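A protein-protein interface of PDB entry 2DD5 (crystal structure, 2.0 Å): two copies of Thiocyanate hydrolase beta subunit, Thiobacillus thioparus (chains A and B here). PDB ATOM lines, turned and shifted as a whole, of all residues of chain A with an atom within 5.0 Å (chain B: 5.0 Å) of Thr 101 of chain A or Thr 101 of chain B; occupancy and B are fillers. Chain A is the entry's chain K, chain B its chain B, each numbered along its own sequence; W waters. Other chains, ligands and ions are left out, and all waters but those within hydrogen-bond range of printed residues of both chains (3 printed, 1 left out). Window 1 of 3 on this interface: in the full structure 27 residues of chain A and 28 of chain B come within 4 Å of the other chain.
OG1 of Thr 101 of chain B sits at hydrogen-bond distance from OG1 of Thr 101 of chain A, 2.7 Å away.
Among the printed residues, pairs that only touch across the chains: Tyr 43 of chain A with Val 102 of chain B, Tyr 43 of chain A with Gly 105 of chain B, Gly 105 of chain A with Tyr 43 of chain B, Gln 100 of chain A with Thr 101 of chain B, Met 106 of chain A with Tyr 43 of chain B, Val 102 of chain A with Tyr 43 of chain B, Thr 101 of chain A with Gln 100 of chain B and Tyr 43 of chain A with Met 106 of chain B.
Of the printed residues of chain B, Gln 100 of chain A touches Thr 101.
Printed residues of chain B within 4 Å of Thr 101 of chain A: Gln 100 (3.6 Å) and Thr 101 (2.7 Å).
Of the printed residues of chain B, Val 102 of chain A touches Tyr 43.
Of the printed residues of chain A, Tyr 43 of chain B touches Val 102 (3.6 Å), Gly 105 (3.6 Å) and Met 106 (3.6 Å).
Of the printed residues of chain A, Thr 101 of chain B touches Gln 100 (3.6 Å) and Thr 101 (2.7 Å).
Of the printed residues of chain A, Gly 105 of chain B touches Tyr 43 (3.5 Å).
Printed residues of chain A within 4 Å of Met 106 of chain B: Tyr 43 (3.7 Å).
The nearest residue of chain B that does not touch Thr 101 of chain A is Tyr 43 of chain B (4.1 Å).
The nearest residue of chain A that does not touch Thr 101 of chain B is Tyr 43 of chain A (4.04 Å).
Of the 9 printed residues of chain B, 6 touch a printed residue of chain A.
Printed residues of chain B that touch a printed residue of chain A: Tyr 43, Gln 100, Thr 101, Val 102, Gly 105 and Met 106.
Hydrophobic or aromatic side chains of chain B that line the printed part of chain A: Tyr 43, Val 102 and Met 106.
Of the 9 printed residues of chain A, 6 touch a printed residue of chain B.
Hydrophobic or aromatic side chains of chain A within 4 Å of the printed part of chain B: Tyr 43, Val 102 and Met 106.
Among the printed residues, 9 pairs touch across the chains.
Tyr 43 of chain A touches Val 102 of chain B, and with the chains exchanged Val 102 of chain A touches Tyr 43 of chain B.
Tyr 43 of chain A touches Gly 105 of chain B, and with the chains exchanged Gly 105 of chain A touches Tyr 43 of chain B.
Tyr 43 of chain A touches Met 106 of chain B, and with the chains exchanged Met 106 of chain A touches Tyr 43 of chain B.
Thr 101 of chain A touches its own counterpart, Thr 101 of chain B.
Positions printed for both chains: 43, 99, 100, 101, 102, 103, 104, 105 and 106.
Water W2 bridges OH of Tyr 43 of chain B (2.7 Å) and O of Gly 105 of chain A (2.7 Å).
Water W3 bridges O of Gly 105 of chain B and OH of Tyr 43 of chain A.
Water W1 bridges the backbone NH of Gly 99 of chain A (3.0 Å) and the backbone NH of Gly 99 of chain B (3.3 Å).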
ATOM      1  N   TYR A  43      20.225 -18.676 -18.898  1.00  0.00           N
ATOM      2  CA  TYR A  43      20.696 -17.637 -17.983  1.00  0.00           C
ATOM      3  C   TYR A  43      19.645 -17.176 -16.974  1.00  0.00           C
ATOM      4  O   TYR A  43      19.986 -16.812 -15.850  1.00  0.00           O
ATOM      5  CB  TYR A  43      21.207 -16.416 -18.761  1.00  0.00           C
ATOM      6  CG  TYR A  43      22.630 -16.548 -19.249  1.00  0.00           C
ATOM      7  CD1 TYR A  43      23.679 -16.764 -18.351  1.00  0.00           C
ATOM      8  CD2 TYR A  43      22.933 -16.453 -20.606  1.00  0.00           C
ATOM      9  CE1 TYR A  43      24.995 -16.882 -18.797  1.00  0.00           C
ATOM     10  CE2 TYR A  43      24.242 -16.570 -21.062  1.00  0.00           C
ATOM     11  CZ  TYR A  43      25.266 -16.785 -20.154  1.00  0.00           C
ATOM     12  OH  TYR A  43      26.558 -16.896 -20.605  1.00  0.00           O
ATOM     13  N   GLY A  99      22.189 -16.691  -7.156  1.00  0.00           N
ATOM     14  CA  GLY A  99      22.842 -16.811  -8.447  1.00  0.00           C
ATOM     15  C   GLY A  99      23.649 -18.086  -8.609  1.00  0.00           C
ATOM     16  O   GLY A  99      24.132 -18.664  -7.637  1.00  0.00           O
ATOM     17  N   GLN A 100      23.808 -18.500  -9.860  1.00  0.00           N
ATOM     18  CA  GLN A 100      24.524 -19.725 -10.213  1.00  0.00           C
ATOM     19  C   GLN A 100      25.903 -19.918  -9.582  1.00  0.00           C
ATOM     20  O   GLN A 100      26.200 -20.986  -9.046  1.00  0.00           O
ATOM     21  CB  GLN A 100      24.662 -19.804 -11.735  1.00  0.00           C
ATOM     22  CG  GLN A 100      25.271 -21.094 -12.248  1.00  0.00           C
ATOM     23  CD  GLN A 100      24.348 -22.283 -12.062  1.00  0.00           C
ATOM     24  OE1 GLN A 100      24.111 -22.739 -10.943  1.00  0.00           O
ATOM     25  NE2 GLN A 100      23.806 -22.781 -13.163  1.00  0.00           N
ATOM     26  N   THR A 101      26.752 -18.898  -9.657  1.00  0.00           N
ATOM     27  CA  THR A 101      28.108 -19.011  -9.121  1.00  0.00           C
ATOM     28  C   THR A 101      28.167 -19.311  -7.629  1.00  0.00           C
ATOM     29  O   THR A 101      28.836 -20.254  -7.207  1.00  0.00           O
ATOM     30  CB  THR A 101      28.931 -17.738  -9.409  1.00  0.00           C
ATOM     31  OG1 THR A 101      29.070 -17.579 -10.826  1.00  0.00           O
ATOM     32  CG2 THR A 101      30.319 -17.834  -8.769  1.00  0.00           C
ATOM     33  N   VAL A 102      27.482 -18.507  -6.825  1.00  0.00           N
ATOM     34  CA  VAL A 102      27.486 -18.737  -5.386  1.00  0.00           C
ATOM     35  C   VAL A 102      26.711 -20.012  -5.044  1.00  0.00           C
ATOM     36  O   VAL A 102      27.062 -20.729  -4.107  1.00  0.00           O
ATOM     37  CB  VAL A 102      26.863 -17.550  -4.625  1.00  0.00           C
ATOM     38  CG1 VAL A 102      26.584 -17.942  -3.170  1.00  0.00           C
ATOM     39  CG2 VAL A 102      27.815 -16.352  -4.665  1.00  0.00           C
ATOM     40  N   TYR A 103      25.661 -20.289  -5.810  1.00  0.00           N
ATOM     41  CA  TYR A 103      24.839 -21.468  -5.569  1.00  0.00           C
ATOM     42  C   TYR A 103      25.647 -22.765  -5.523  1.00  0.00           C
ATOM     43  O   TYR A 103      25.418 -23.613  -4.660  1.00  0.00           O
ATOM     44  CB  TYR A 103      23.747 -21.585  -6.637  1.00  0.00           C
ATOM     45  CG  TYR A 103      22.768 -22.700  -6.340  1.00  0.00           C
ATOM     46  CD1 TYR A 103      21.988 -22.672  -5.181  1.00  0.00           C
ATOM     47  CD2 TYR A 103      22.663 -23.809  -7.182  1.00  0.00           C
ATOM     48  CE1 TYR A 103      21.130 -23.721  -4.860  1.00  0.00           C
ATOM     49  CE2 TYR A 103      21.803 -24.875  -6.868  1.00  0.00           C
ATOM     50  CZ  TYR A 103      21.045 -24.822  -5.707  1.00  0.00           C
ATOM     51  OH  TYR A 103      20.218 -25.870  -5.366  1.00  0.00           O
ATOM     52  N   LEU A 104      26.598 -22.922  -6.436  1.00  0.00           N
ATOM     53  CA  LEU A 104      27.402 -24.140  -6.465  1.00  0.00           C
ATOM     54  C   LEU A 104      28.828 -23.957  -5.947  1.00  0.00           C
ATOM     55  O   LEU A 104      29.520 -24.936  -5.656  1.00  0.00           O
ATOM     56  CB  LEU A 104      27.417 -24.712  -7.887  1.00  0.00           C
ATOM     57  CG  LEU A 104      26.063 -25.282  -8.335  1.00  0.00           C
ATOM     58  CD1 LEU A 104      26.092 -25.633  -9.819  1.00  0.00           C
ATOM     59  CD2 LEU A 104      25.749 -26.524  -7.504  1.00  0.00           C
ATOM     60  N   GLY A 105      29.261 -22.708  -5.808  1.00  0.00           N
ATOM     61  CA  GLY A 105      30.610 -22.456  -5.327  1.00  0.00           C
ATOM     62  C   GLY A 105      30.756 -22.447  -3.815  1.00  0.00           C
ATOM     63  O   GLY A 105      31.795 -22.839  -3.280  1.00  0.00           O
ATOM     64  N   MET A 106      29.719 -22.000  -3.117  1.00  0.00           N
ATOM     65  CA  MET A 106      29.761 -21.931  -1.659  1.00  0.00           C
ATOM     66  C   MET A 106      29.085 -23.141  -1.025  1.00  0.00           C
ATOM     67  O   MET A 106      28.353 -23.863  -1.690  1.00  0.00           O
ATOM     68  CB  MET A 106      29.086 -20.643  -1.185  1.00  0.00           C
ATOM     69  CG  MET A 106      29.919 -19.389  -1.449  1.00  0.00           C
ATOM     70  SD  MET A 106      31.335 -19.271  -0.308  1.00  0.00           S
ATOM     71  CE  MET A 106      30.546 -18.416   1.049  1.00  0.00           C
ATOM     72  N   TYR B  43      33.977 -15.089  -3.247  1.00  0.00           N
ATOM     73  CA  TYR B  43      32.578 -15.446  -3.487  1.00  0.00           C
ATOM     74  C   TYR B  43      31.589 -14.403  -2.986  1.00  0.00           C
ATOM     75  O   TYR B  43      30.515 -14.243  -3.566  1.00  0.00           O
ATOM     76  CB  TYR B  43      32.236 -16.803  -2.847  1.00  0.00           C
ATOM     77  CG  TYR B  43      32.684 -18.001  -3.657  1.00  0.00           C
ATOM     78  CD1 TYR B  43      33.542 -18.956  -3.113  1.00  0.00           C
ATOM     79  CD2 TYR B  43      32.246 -18.182  -4.971  1.00  0.00           C
ATOM     80  CE1 TYR B  43      33.955 -20.060  -3.856  1.00  0.00           C
ATOM     81  CE2 TYR B  43      32.653 -19.282  -5.721  1.00  0.00           C
ATOM     82  CZ  TYR B  43      33.507 -20.214  -5.158  1.00  0.00           C
ATOM     83  OH  TYR B  43      33.920 -21.288  -5.898  1.00  0.00           O
ATOM     84  N   GLY B  99      24.247 -11.510  -9.438  1.00  0.00           N
ATOM     85  CA  GLY B  99      25.251 -12.555  -9.356  1.00  0.00           C
ATOM     86  C   GLY B  99      26.238 -12.588 -10.507  1.00  0.00           C
ATOM     87  O   GLY B  99      25.931 -12.194 -11.633  1.00  0.00           O
ATOM     88  N   GLN B 100      27.427 -13.094 -10.204  1.00  0.00           N
ATOM     89  CA  GLN B 100      28.539 -13.202 -11.141  1.00  0.00           C
ATOM     90  C   GLN B 100      28.215 -13.783 -12.517  1.00  0.00           C
ATOM     91  O   GLN B 100      28.595 -13.212 -13.534  1.00  0.00           O
ATOM     92  CB  GLN B 100      29.653 -14.032 -10.496  1.00  0.00           C
ATOM     93  CG  GLN B 100      30.937 -14.108 -11.293  1.00  0.00           C
ATOM     94  CD  GLN B 100      31.689 -12.790 -11.312  1.00  0.00           C
ATOM     95  OE1 GLN B 100      31.250 -11.818 -11.926  1.00  0.00           O
ATOM     96  NE2 GLN B 100      32.822 -12.751 -10.631  1.00  0.00           N
ATOM     97  N   THR B 101      27.517 -14.917 -12.555  1.00  0.00           N
ATOM     98  CA  THR B 101      27.196 -15.558 -13.835  1.00  0.00           C
ATOM     99  C   THR B 101      26.362 -14.690 -14.770  1.00  0.00           C
ATOM    100  O   THR B 101      26.741 -14.466 -15.924  1.00  0.00           O
ATOM    101  CB  THR B 101      26.474 -16.909 -13.616  1.00  0.00           C
ATOM    102  OG1 THR B 101      27.358 -17.805 -12.927  1.00  0.00           O
ATOM    103  CG2 THR B 101      26.072 -17.532 -14.961  1.00  0.00           C
ATOM    104  N   VAL B 102      25.223 -14.210 -14.289  1.00  0.00           N
ATOM    105  CA  VAL B 102      24.378 -13.360 -15.117  1.00  0.00           C
ATOM    106  C   VAL B 102      25.054 -12.013 -15.376  1.00  0.00           C
ATOM    107  O   VAL B 102      24.906 -11.432 -16.452  1.00  0.00           O
ATOM    108  CB  VAL B 102      23.009 -13.131 -14.450  1.00  0.00           C
ATOM    109  CG1 VAL B 102      22.248 -12.002 -15.157  1.00  0.00           C
ATOM    110  CG2 VAL B 102      22.195 -14.425 -14.509  1.00  0.00           C
ATOM    111  N   TYR B 103      25.816 -11.536 -14.397  1.00  0.00           N
ATOM    112  CA  TYR B 103      26.494 -10.250 -14.524  1.00  0.00           C
ATOM    113  C   TYR B 103      27.383 -10.151 -15.762  1.00  0.00           C
ATOM    114  O   TYR B 103      27.406  -9.121 -16.436  1.00  0.00           O
ATOM    115  CB  TYR B 103      27.333  -9.954 -13.276  1.00  0.00           C
ATOM    116  CG  TYR B 103      27.937  -8.569 -13.296  1.00  0.00           C
ATOM    117  CD1 TYR B 103      27.122  -7.432 -13.252  1.00  0.00           C
ATOM    118  CD2 TYR B 103      29.313  -8.390 -13.414  1.00  0.00           C
ATOM    119  CE1 TYR B 103      27.667  -6.151 -13.332  1.00  0.00           C
ATOM    120  CE2 TYR B 103      29.870  -7.113 -13.493  1.00  0.00           C
ATOM    121  CZ  TYR B 103      29.040  -6.000 -13.452  1.00  0.00           C
ATOM    122  OH  TYR B 103      29.587  -4.740 -13.545  1.00  0.00           O
ATOM    123  N   LEU B 104      28.122 -11.212 -16.062  1.00  0.00           N
ATOM    124  CA  LEU B 104      28.999 -11.193 -17.228  1.00  0.00           C
ATOM    125  C   LEU B 104      28.470 -12.018 -18.393  1.00  0.00           C
ATOM    126  O   LEU B 104      28.943 -11.882 -19.520  1.00  0.00           O
ATOM    127  CB  LEU B 104      30.404 -11.665 -16.834  1.00  0.00           C
ATOM    128  CG  LEU B 104      31.157 -10.677 -15.928  1.00  0.00           C
ATOM    129  CD1 LEU B 104      32.452 -11.295 -15.416  1.00  0.00           C
ATOM    130  CD2 LEU B 104      31.450  -9.407 -16.709  1.00  0.00           C
ATOM    131  N   GLY B 105      27.472 -12.855 -18.131  1.00  0.00           N
ATOM    132  CA  GLY B 105      26.927 -13.687 -19.188  1.00  0.00           C
ATOM    133  C   GLY B 105      25.843 -13.035 -20.027  1.00  0.00           C
ATOM    134  O   GLY B 105      25.714 -13.325 -21.217  1.00  0.00           O
ATOM    135  N   MET B 106      25.055 -12.162 -19.410  1.00  0.00           N
ATOM    136  CA  MET B 106      23.971 -11.483 -20.108  1.00  0.00           C
ATOM    137  C   MET B 106      24.382 -10.088 -20.574  1.00  0.00           C
ATOM    138  O   MET B 106      25.420  -9.564 -20.164  1.00  0.00           O
ATOM    139  CB  MET B 106      22.745 -11.396 -19.199  1.00  0.00           C
ATOM    140  CG  MET B 106      22.003 -12.724 -19.028  1.00  0.00           C
ATOM    141  SD  MET B 106      21.074 -13.212 -20.515  1.00  0.00           S
ATOM    142  CE  MET B 106      19.555 -12.312 -20.252  1.00  0.00           C
HETATM  143  O   HOH W   1      22.549 -13.733  -7.771  1.00  0.00           O
HETATM  144  O   HOH W   2      34.316 -23.327  -4.222  1.00  0.00           O
HETATM  145  O   HOH W   3      26.823 -15.205 -22.836  1.00  0.00           O
